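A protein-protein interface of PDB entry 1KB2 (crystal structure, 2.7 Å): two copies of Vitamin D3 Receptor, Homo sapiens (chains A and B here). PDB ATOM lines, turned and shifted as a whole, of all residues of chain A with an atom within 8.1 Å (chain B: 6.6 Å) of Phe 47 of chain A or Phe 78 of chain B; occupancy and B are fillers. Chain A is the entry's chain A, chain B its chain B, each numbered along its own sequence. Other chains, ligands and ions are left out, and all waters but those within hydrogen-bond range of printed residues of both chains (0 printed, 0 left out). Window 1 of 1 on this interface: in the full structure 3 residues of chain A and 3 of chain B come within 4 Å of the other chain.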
ATOM      1  N   THR A  44      13.596   7.000 -25.518  1.00  0.00           N
ATOM      2  CA  THR A  44      14.300   7.019 -24.238  1.00  0.00           C
ATOM      3  C   THR A  44      13.701   6.033 -23.236  1.00  0.00           C
ATOM      4  O   THR A  44      12.535   6.173 -22.876  1.00  0.00           O
ATOM      5  CB  THR A  44      14.279   8.461 -23.611  1.00  0.00           C
ATOM      6  OG1 THR A  44      15.209   9.303 -24.316  1.00  0.00           O
ATOM      7  CG2 THR A  44      14.635   8.430 -22.123  1.00  0.00           C
ATOM      8  N   CYS A  45      14.503   5.061 -22.777  1.00  0.00           N
ATOM      9  CA  CYS A  45      14.028   4.081 -21.814  1.00  0.00           C
ATOM     10  C   CYS A  45      13.600   4.720 -20.476  1.00  0.00           C
ATOM     11  O   CYS A  45      14.323   5.504 -19.898  1.00  0.00           O
ATOM     12  CB  CYS A  45      15.107   3.042 -21.587  1.00  0.00           C
ATOM     13  SG  CYS A  45      14.558   1.658 -20.582  1.00  0.00           S
ATOM     14  N   PRO A  46      12.416   4.381 -19.956  1.00  0.00           N
ATOM     15  CA  PRO A  46      11.945   4.958 -18.683  1.00  0.00           C
ATOM     16  C   PRO A  46      12.527   4.268 -17.460  1.00  0.00           C
ATOM     17  O   PRO A  46      12.321   4.693 -16.319  1.00  0.00           O
ATOM     18  CB  PRO A  46      10.426   4.744 -18.719  1.00  0.00           C
ATOM     19  CG  PRO A  46      10.145   4.284 -20.131  1.00  0.00           C
ATOM     20  CD  PRO A  46      11.374   3.562 -20.575  1.00  0.00           C
ATOM     21  N   PHE A  47      13.232   3.179 -17.701  1.00  0.00           N
ATOM     22  CA  PHE A  47      13.791   2.394 -16.624  1.00  0.00           C
ATOM     23  C   PHE A  47      15.294   2.387 -16.550  1.00  0.00           C
ATOM     24  O   PHE A  47      15.896   3.394 -16.214  1.00  0.00           O
ATOM     25  CB  PHE A  47      13.282   0.971 -16.747  1.00  0.00           C
ATOM     26  CG  PHE A  47      11.809   0.888 -16.843  1.00  0.00           C
ATOM     27  CD1 PHE A  47      11.046   0.611 -15.727  1.00  0.00           C
ATOM     28  CD2 PHE A  47      11.172   1.109 -18.061  1.00  0.00           C
ATOM     29  CE1 PHE A  47       9.656   0.553 -15.825  1.00  0.00           C
ATOM     30  CE2 PHE A  47       9.783   1.053 -18.175  1.00  0.00           C
ATOM     31  CZ  PHE A  47       9.024   0.773 -17.060  1.00  0.00           C
ATOM     32  N   ASN A  48      15.887   1.246 -16.891  1.00  0.00           N
ATOM     33  CA  ASN A  48      17.322   1.059 -16.815  1.00  0.00           C
ATOM     34  C   ASN A  48      18.067   0.832 -18.116  1.00  0.00           C
ATOM     35  O   ASN A  48      19.296   0.667 -18.072  1.00  0.00           O
ATOM     36  CB  ASN A  48      17.640  -0.095 -15.873  1.00  0.00           C
ATOM     37  CG  ASN A  48      16.937   0.043 -14.555  1.00  0.00           C
ATOM     38  OD1 ASN A  48      17.196   0.985 -13.806  1.00  0.00           O
ATOM     39  ND2 ASN A  48      16.025  -0.883 -14.260  1.00  0.00           N
ATOM     40  N   GLY A  49      17.369   0.807 -19.257  1.00  0.00           N
ATOM     41  CA  GLY A  49      18.056   0.621 -20.524  1.00  0.00           C
ATOM     42  C   GLY A  49      18.339  -0.814 -20.908  1.00  0.00           C
ATOM     43  O   GLY A  49      19.007  -1.094 -21.902  1.00  0.00           O
ATOM     44  N   ASP A  50      17.826  -1.746 -20.125  1.00  0.00           N
ATOM     45  CA  ASP A  50      18.022  -3.150 -20.443  1.00  0.00           C
ATOM     46  C   ASP A  50      16.743  -3.939 -20.229  1.00  0.00           C
ATOM     47  O   ASP A  50      16.765  -5.051 -19.655  1.00  0.00           O
ATOM     48  CB  ASP A  50      19.120  -3.730 -19.589  1.00  0.00           C
ATOM     49  CG  ASP A  50      18.960  -3.364 -18.160  1.00  0.00           C
ATOM     50  OD1 ASP A  50      17.943  -2.715 -17.829  1.00  0.00           O
ATOM     51  OD2 ASP A  50      19.849  -3.713 -17.365  1.00  0.00           O
ATOM     52  N   CYS A  51      15.637  -3.348 -20.691  1.00  0.00           N
ATOM     53  CA  CYS A  51      14.304  -3.952 -20.607  1.00  0.00           C
ATOM     54  C   CYS A  51      14.259  -5.311 -21.310  1.00  0.00           C
ATOM     55  O   CYS A  51      14.866  -5.509 -22.386  1.00  0.00           O
ATOM     56  CB  CYS A  51      13.271  -3.031 -21.241  1.00  0.00           C
ATOM     57  SG  CYS A  51      12.909  -1.480 -20.397  1.00  0.00           S
ATOM     58  N   ASN A  57       4.941  -7.046 -23.580  1.00  0.00           N
ATOM     59  CA  ASN A  57       5.330  -5.729 -23.115  1.00  0.00           C
ATOM     60  C   ASN A  57       6.036  -4.847 -24.136  1.00  0.00           C
ATOM     61  O   ASN A  57       6.315  -3.692 -23.838  1.00  0.00           O
ATOM     62  CB  ASN A  57       6.265  -5.856 -21.929  1.00  0.00           C
ATOM     63  CG  ASN A  57       7.545  -6.633 -22.265  1.00  0.00           C
ATOM     64  OD1 ASN A  57       7.906  -6.815 -23.436  1.00  0.00           O
ATOM     65  ND2 ASN A  57       8.243  -7.079 -21.231  1.00  0.00           N
ATOM     66  N   ARG A  59       5.366  -2.901 -26.413  1.00  0.00           N
ATOM     67  CA  ARG A  59       4.926  -1.539 -26.725  1.00  0.00           C
ATOM     68  C   ARG A  59       5.300  -0.567 -25.620  1.00  0.00           C
ATOM     69  O   ARG A  59       5.266   0.646 -25.821  1.00  0.00           O
ATOM     70  CB  ARG A  59       3.427  -1.510 -26.961  1.00  0.00           C
ATOM     71  CG  ARG A  59       2.993  -2.395 -28.128  1.00  0.00           C
ATOM     72  CD  ARG A  59       1.509  -2.288 -28.431  1.00  0.00           C
ATOM     73  NE  ARG A  59       0.735  -2.918 -27.378  1.00  0.00           N
ATOM     74  CZ  ARG A  59       0.590  -4.237 -27.250  1.00  0.00           C
ATOM     75  NH1 ARG A  59       1.161  -5.093 -28.124  1.00  0.00           N
ATOM     76  NH2 ARG A  59      -0.116  -4.707 -26.220  1.00  0.00           N
ATOM     77  N   HIS A  60       5.689  -1.112 -24.468  1.00  0.00           N
ATOM     78  CA  HIS A  60       6.065  -0.323 -23.299  1.00  0.00           C
ATOM     79  C   HIS A  60       7.456   0.304 -23.398  1.00  0.00           C
ATOM     80  O   HIS A  60       7.664   1.428 -22.940  1.00  0.00           O
ATOM     81  CB  HIS A  60       5.960  -1.159 -22.000  1.00  0.00           C
ATOM     82  CG  HIS A  60       4.588  -1.731 -21.741  1.00  0.00           C
ATOM     83  ND1 HIS A  60       3.416  -1.047 -22.036  1.00  0.00           N
ATOM     84  CD2 HIS A  60       4.205  -2.938 -21.239  1.00  0.00           C
ATOM     85  CE1 HIS A  60       2.377  -1.812 -21.735  1.00  0.00           C
ATOM     86  NE2 HIS A  60       2.828  -2.964 -21.250  1.00  0.00           N
ATOM     87  N   CYS A  61       8.439  -0.385 -23.944  1.00  0.00           N
ATOM     88  CA  CYS A  61       9.680   0.331 -24.062  1.00  0.00           C
ATOM     89  C   CYS A  61      10.196   0.368 -25.494  1.00  0.00           C
ATOM     90  O   CYS A  61      10.880  -0.566 -25.960  1.00  0.00           O
ATOM     91  CB  CYS A  61      10.755  -0.212 -23.128  1.00  0.00           C
ATOM     92  SG  CYS A  61      12.260   0.902 -23.134  1.00  0.00           S
ATOM     93  N   GLN A  62       9.882   1.451 -26.200  1.00  0.00           N
ATOM     94  CA  GLN A  62      10.346   1.574 -27.576  1.00  0.00           C
ATOM     95  C   GLN A  62      11.858   1.708 -27.655  1.00  0.00           C
ATOM     96  O   GLN A  62      12.488   1.109 -28.529  1.00  0.00           O
ATOM     97  CB  GLN A  62       9.685   2.753 -28.231  1.00  0.00           C
ATOM     98  CG  GLN A  62       8.394   2.981 -27.592  1.00  0.00           C
ATOM     99  CD  GLN A  62       7.600   4.030 -28.280  1.00  0.00           C
ATOM    100  OE1 GLN A  62       7.949   5.221 -28.263  1.00  0.00           O
ATOM    101  NE2 GLN A  62       6.503   3.602 -28.902  1.00  0.00           N
ATOM    102  N   ALA A  63      12.454   2.474 -26.750  1.00  0.00           N
ATOM    103  CA  ALA A  63      13.906   2.624 -26.775  1.00  0.00           C
ATOM    104  C   ALA A  63      14.561   1.277 -26.790  1.00  0.00           C
ATOM    105  O   ALA A  63      15.409   1.009 -27.644  1.00  0.00           O
ATOM    106  CB  ALA A  63      14.378   3.380 -25.601  1.00  0.00           C
ATOM    107  N   CYS A  64      14.149   0.408 -25.866  1.00  0.00           N
ATOM    108  CA  CYS A  64      14.740  -0.928 -25.783  1.00  0.00           C
ATOM    109  C   CYS A  64      14.366  -1.798 -26.945  1.00  0.00           C
ATOM    110  O   CYS A  64      15.228  -2.523 -27.443  1.00  0.00           O
ATOM    111  CB  CYS A  64      14.402  -1.638 -24.454  1.00  0.00           C
ATOM    112  SG  CYS A  64      15.348  -1.029 -22.990  1.00  0.00           S
ATOM    113  N   HIS B  20      -4.451   1.340 -18.750  1.00  0.00           N
ATOM    114  CA  HIS B  20      -3.954   2.686 -18.555  1.00  0.00           C
ATOM    115  C   HIS B  20      -2.756   2.555 -17.666  1.00  0.00           C
ATOM    116  O   HIS B  20      -2.826   1.958 -16.599  1.00  0.00           O
ATOM    117  CB  HIS B  20      -5.031   3.571 -17.917  1.00  0.00           C
ATOM    118  CG  HIS B  20      -6.238   3.746 -18.778  1.00  0.00           C
ATOM    119  ND1 HIS B  20      -6.238   4.546 -19.899  1.00  0.00           N
ATOM    120  CD2 HIS B  20      -7.457   3.160 -18.733  1.00  0.00           C
ATOM    121  CE1 HIS B  20      -7.405   4.446 -20.507  1.00  0.00           C
ATOM    122  NE2 HIS B  20      -8.161   3.610 -19.822  1.00  0.00           N
ATOM    123  N   PHE B  21      -1.640   3.103 -18.126  1.00  0.00           N
ATOM    124  CA  PHE B  21      -0.400   3.000 -17.387  1.00  0.00           C
ATOM    125  C   PHE B  21      -0.160   1.538 -16.996  1.00  0.00           C
ATOM    126  O   PHE B  21       0.358   1.238 -15.931  1.00  0.00           O
ATOM    127  CB  PHE B  21      -0.482   3.932 -16.204  1.00  0.00           C
ATOM    128  CG  PHE B  21      -0.762   5.337 -16.622  1.00  0.00           C
ATOM    129  CD1 PHE B  21       0.237   6.107 -17.227  1.00  0.00           C
ATOM    130  CD2 PHE B  21      -2.055   5.857 -16.546  1.00  0.00           C
ATOM    131  CE1 PHE B  21      -0.047   7.329 -17.739  1.00  0.00           C
ATOM    132  CE2 PHE B  21      -2.337   7.100 -17.068  1.00  0.00           C
ATOM    133  CZ  PHE B  21      -1.345   7.833 -17.664  1.00  0.00           C
ATOM    134  N   ASN B  22      -0.568   0.631 -17.882  1.00  0.00           N
ATOM    135  CA  ASN B  22      -0.379  -0.792 -17.693  1.00  0.00           C
ATOM    136  C   ASN B  22      -1.286  -1.476 -16.738  1.00  0.00           C
ATOM    137  O   ASN B  22      -0.887  -2.471 -16.184  1.00  0.00           O
ATOM    138  CB  ASN B  22       1.063  -1.078 -17.274  1.00  0.00           C
ATOM    139  CG  ASN B  22       1.471  -2.535 -17.486  1.00  0.00           C
ATOM    140  OD1 ASN B  22       1.123  -3.160 -18.505  1.00  0.00           O
ATOM    141  ND2 ASN B  22       2.238  -3.072 -16.538  1.00  0.00           N
ATOM    142  N   ALA B  23      -2.503  -0.969 -16.551  1.00  0.00           N
ATOM    143  CA  ALA B  23      -3.478  -1.585 -15.630  1.00  0.00           C
ATOM    144  C   ALA B  23      -4.924  -1.372 -16.078  1.00  0.00           C
ATOM    145  O   ALA B  23      -5.263  -0.295 -16.559  1.00  0.00           O
ATOM    146  CB  ALA B  23      -3.288  -1.025 -14.225  1.00  0.00           C
ATOM    147  N   GLY B  73      -0.332  -2.217 -10.330  1.00  0.00           N
ATOM    148  CA  GLY B  73       0.403  -2.120 -11.568  1.00  0.00           C
ATOM    149  C   GLY B  73       0.637  -0.783 -12.219  1.00  0.00           C
ATOM    150  O   GLY B  73       1.601  -0.627 -12.937  1.00  0.00           O
ATOM    151  N   MET B  74      -0.207   0.198 -11.988  1.00  0.00           N
ATOM    152  CA  MET B  74      -0.008   1.479 -12.644  1.00  0.00           C
ATOM    153  C   MET B  74       1.387   2.074 -12.522  1.00  0.00           C
ATOM    154  O   MET B  74       1.873   2.420 -11.444  1.00  0.00           O
ATOM    155  CB  MET B  74      -1.080   2.450 -12.161  1.00  0.00           C
ATOM    156  CG  MET B  74      -2.455   1.891 -12.501  1.00  0.00           C
ATOM    157  SD  MET B  74      -3.829   2.911 -12.093  1.00  0.00           S
ATOM    158  CE  MET B  74      -3.492   4.330 -13.112  1.00  0.00           C
ATOM    159  N   MET B  75       2.055   2.224 -13.645  1.00  0.00           N
ATOM    160  CA  MET B  75       3.385   2.761 -13.544  1.00  0.00           C
ATOM    161  C   MET B  75       3.645   4.196 -13.943  1.00  0.00           C
ATOM    162  O   MET B  75       3.440   4.600 -15.081  1.00  0.00           O
ATOM    163  CB  MET B  75       4.359   1.795 -14.228  1.00  0.00           C
ATOM    164  CG  MET B  75       4.946   0.827 -13.183  1.00  0.00           C
ATOM    165  SD  MET B  75       5.545  -0.717 -13.800  1.00  0.00           S
ATOM    166  CE  MET B  75       3.912  -1.639 -14.152  1.00  0.00           C
ATOM    167  N   LYS B  76       4.108   4.964 -12.971  1.00  0.00           N
ATOM    168  CA  LYS B  76       4.401   6.351 -13.222  1.00  0.00           C
ATOM    169  C   LYS B  76       5.352   6.467 -14.432  1.00  0.00           C
ATOM    170  O   LYS B  76       5.366   7.510 -15.078  1.00  0.00           O
ATOM    171  CB  LYS B  76       5.010   7.010 -11.964  1.00  0.00           C
ATOM    172  CG  LYS B  76       6.562   6.956 -11.861  1.00  0.00           C
ATOM    173  CD  LYS B  76       7.151   7.116 -10.428  1.00  0.00           C
ATOM    174  CE  LYS B  76       7.353   5.775  -9.676  1.00  0.00           C
ATOM    175  NZ  LYS B  76       6.160   5.136  -8.999  1.00  0.00           N
ATOM    176  N   GLU B  77       6.117   5.418 -14.766  1.00  0.00           N
ATOM    177  CA  GLU B  77       7.063   5.486 -15.903  1.00  0.00           C
ATOM    178  C   GLU B  77       6.414   5.597 -17.264  1.00  0.00           C
ATOM    179  O   GLU B  77       7.019   6.102 -18.217  1.00  0.00           O
ATOM    180  CB  GLU B  77       7.994   4.283 -15.956  1.00  0.00           C
ATOM    181  CG  GLU B  77       8.906   4.147 -14.782  1.00  0.00           C
ATOM    182  CD  GLU B  77       8.190   3.660 -13.535  1.00  0.00           C
ATOM    183  OE1 GLU B  77       7.456   2.644 -13.603  1.00  0.00           O
ATOM    184  OE2 GLU B  77       8.380   4.287 -12.471  1.00  0.00           O
ATOM    185  N   PHE B  78       5.190   5.105 -17.366  1.00  0.00           N
ATOM    186  CA  PHE B  78       4.471   5.189 -18.615  1.00  0.00           C
ATOM    187  C   PHE B  78       3.873   6.575 -18.851  1.00  0.00           C
ATOM    188  O   PHE B  78       3.267   6.806 -19.886  1.00  0.00           O
ATOM    189  CB  PHE B  78       3.383   4.137 -18.643  1.00  0.00           C
ATOM    190  CG  PHE B  78       3.903   2.738 -18.698  1.00  0.00           C
ATOM    191  CD1 PHE B  78       3.041   1.650 -18.534  1.00  0.00           C
ATOM    192  CD2 PHE B  78       5.248   2.490 -18.947  1.00  0.00           C
ATOM    193  CE1 PHE B  78       3.505   0.336 -18.619  1.00  0.00           C
ATOM    194  CE2 PHE B  78       5.722   1.182 -19.034  1.00  0.00           C
ATOM    195  CZ  PHE B  78       4.840   0.102 -18.866  1.00  0.00           C
ATOM    196  N   ILE B  79       4.038   7.496 -17.898  1.00  0.00           N
ATOM    197  CA  ILE B  79       3.503   8.862 -18.050  1.00  0.00           C
ATOM    198  C   ILE B  79       4.465   9.661 -18.901  1.00  0.00           C
ATOM    199  O   ILE B  79       5.666   9.594 -18.697  1.00  0.00           O
ATOM    200  CB  ILE B  79       3.318   9.589 -16.707  1.00  0.00           C
ATOM    201  CG1 ILE B  79       2.474   8.755 -15.768  1.00  0.00           C
ATOM    202  CG2 ILE B  79       2.552  10.836 -16.930  1.00  0.00           C
ATOM    203  CD1 ILE B  79       2.228   9.406 -14.458  1.00  0.00           C
ATOM    204  N   LEU B  80       3.953  10.419 -19.855  1.00  0.00           N
ATOM    205  CA  LEU B  80       4.871  11.144 -20.708  1.00  0.00           C
ATOM    206  C   LEU B  80       5.558  12.270 -19.969  1.00  0.00           C
ATOM    207  O   LEU B  80       4.903  13.088 -19.303  1.00  0.00           O
ATOM    208  CB  LEU B  80       4.178  11.648 -21.986  1.00  0.00           C
ATOM    209  CG  LEU B  80       3.824  10.614 -23.077  1.00  0.00           C
ATOM    210  CD1 LEU B  80       4.213  11.172 -24.424  1.00  0.00           C
ATOM    211  CD2 LEU B  80       4.538   9.272 -22.864  1.00  0.00           C
ATOM    212  N   THR B  81       6.891  12.273 -20.096  1.00  0.00           N
ATOM    213  CA  THR B  81       7.783  13.243 -19.460  1.00  0.00           C
ATOM    214  C   THR B  81       7.575  14.649 -20.012  1.00  0.00           C
ATOM    215  O   THR B  81       7.326  14.827 -21.200  1.00  0.00           O
ATOM    216  CB  THR B  81       9.305  12.823 -19.633  1.00  0.00           C
ATOM    217  OG1 THR B  81       9.771  13.126 -20.958  1.00  0.00           O
ATOM    218  CG2 THR B  81       9.478  11.316 -19.392  1.00  0.00           C
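Of the 13 printed residues of chain B, 3 touch a printed residue of chain A.
Of the 15 printed residues of chain A, 3 touch a printed residue of chain B.
Printed residues of chain A that touch a printed residue of chain B: Pro 46, Phe 47 and His 60.
Hydrophobic or aromatic side chains of chain A that line the printed part of chain B: Pro 46, Phe 47 and His 60.
Phe 78 of chain B touches two residues of chain A.
Of the printed residues of chain B, Pro 46 of chain A touches Glu 77 (3.7 Å).
Printed residues of chain A within 4 Å of Glu 77 of chain B: Pro 46 and Phe 47.
Printed residues of chain A within 4 Å of Asn 22 of chain B: His 60.
Of the printed residues of chain B, His 60 of chain A touches Asn 22 (3.2 Å) and Phe 78 (3.4 Å).
His 20 of chain B touches none of the printed residues of chain A.
The nearest residue of chain B that does not touch Phe 47 of chain A is Met 75 of chain B (4.8 Å).
The nearest residue of chain A that does not touch Phe 78 of chain B is Pro 46 of chain A (5.3 Å).
The side-chain sulfur (SG) of Cys 45 of chain A sits close to the backbone NH (N) of Phe 47 of chain A, at 3.5 Å.
No position is printed for both chains.
Glu 77 of chain B touches Pro 46 of chain A.
Phe 47 of chain A touches Glu 77 of chain B.
Phe 78 of chain B touches Phe 47 of chain A (CE2 to CZ, 3.9 Å).
Phe 78 of chain B touches His 60 of chain A (CZ to CG, 3.4 Å).
A ring nitrogen (NE2) of His 60 of chain A sits at hydrogen-bond distance from the side-chain amide oxygen (OD1) of Asn 22 of chain B (3.2 Å).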
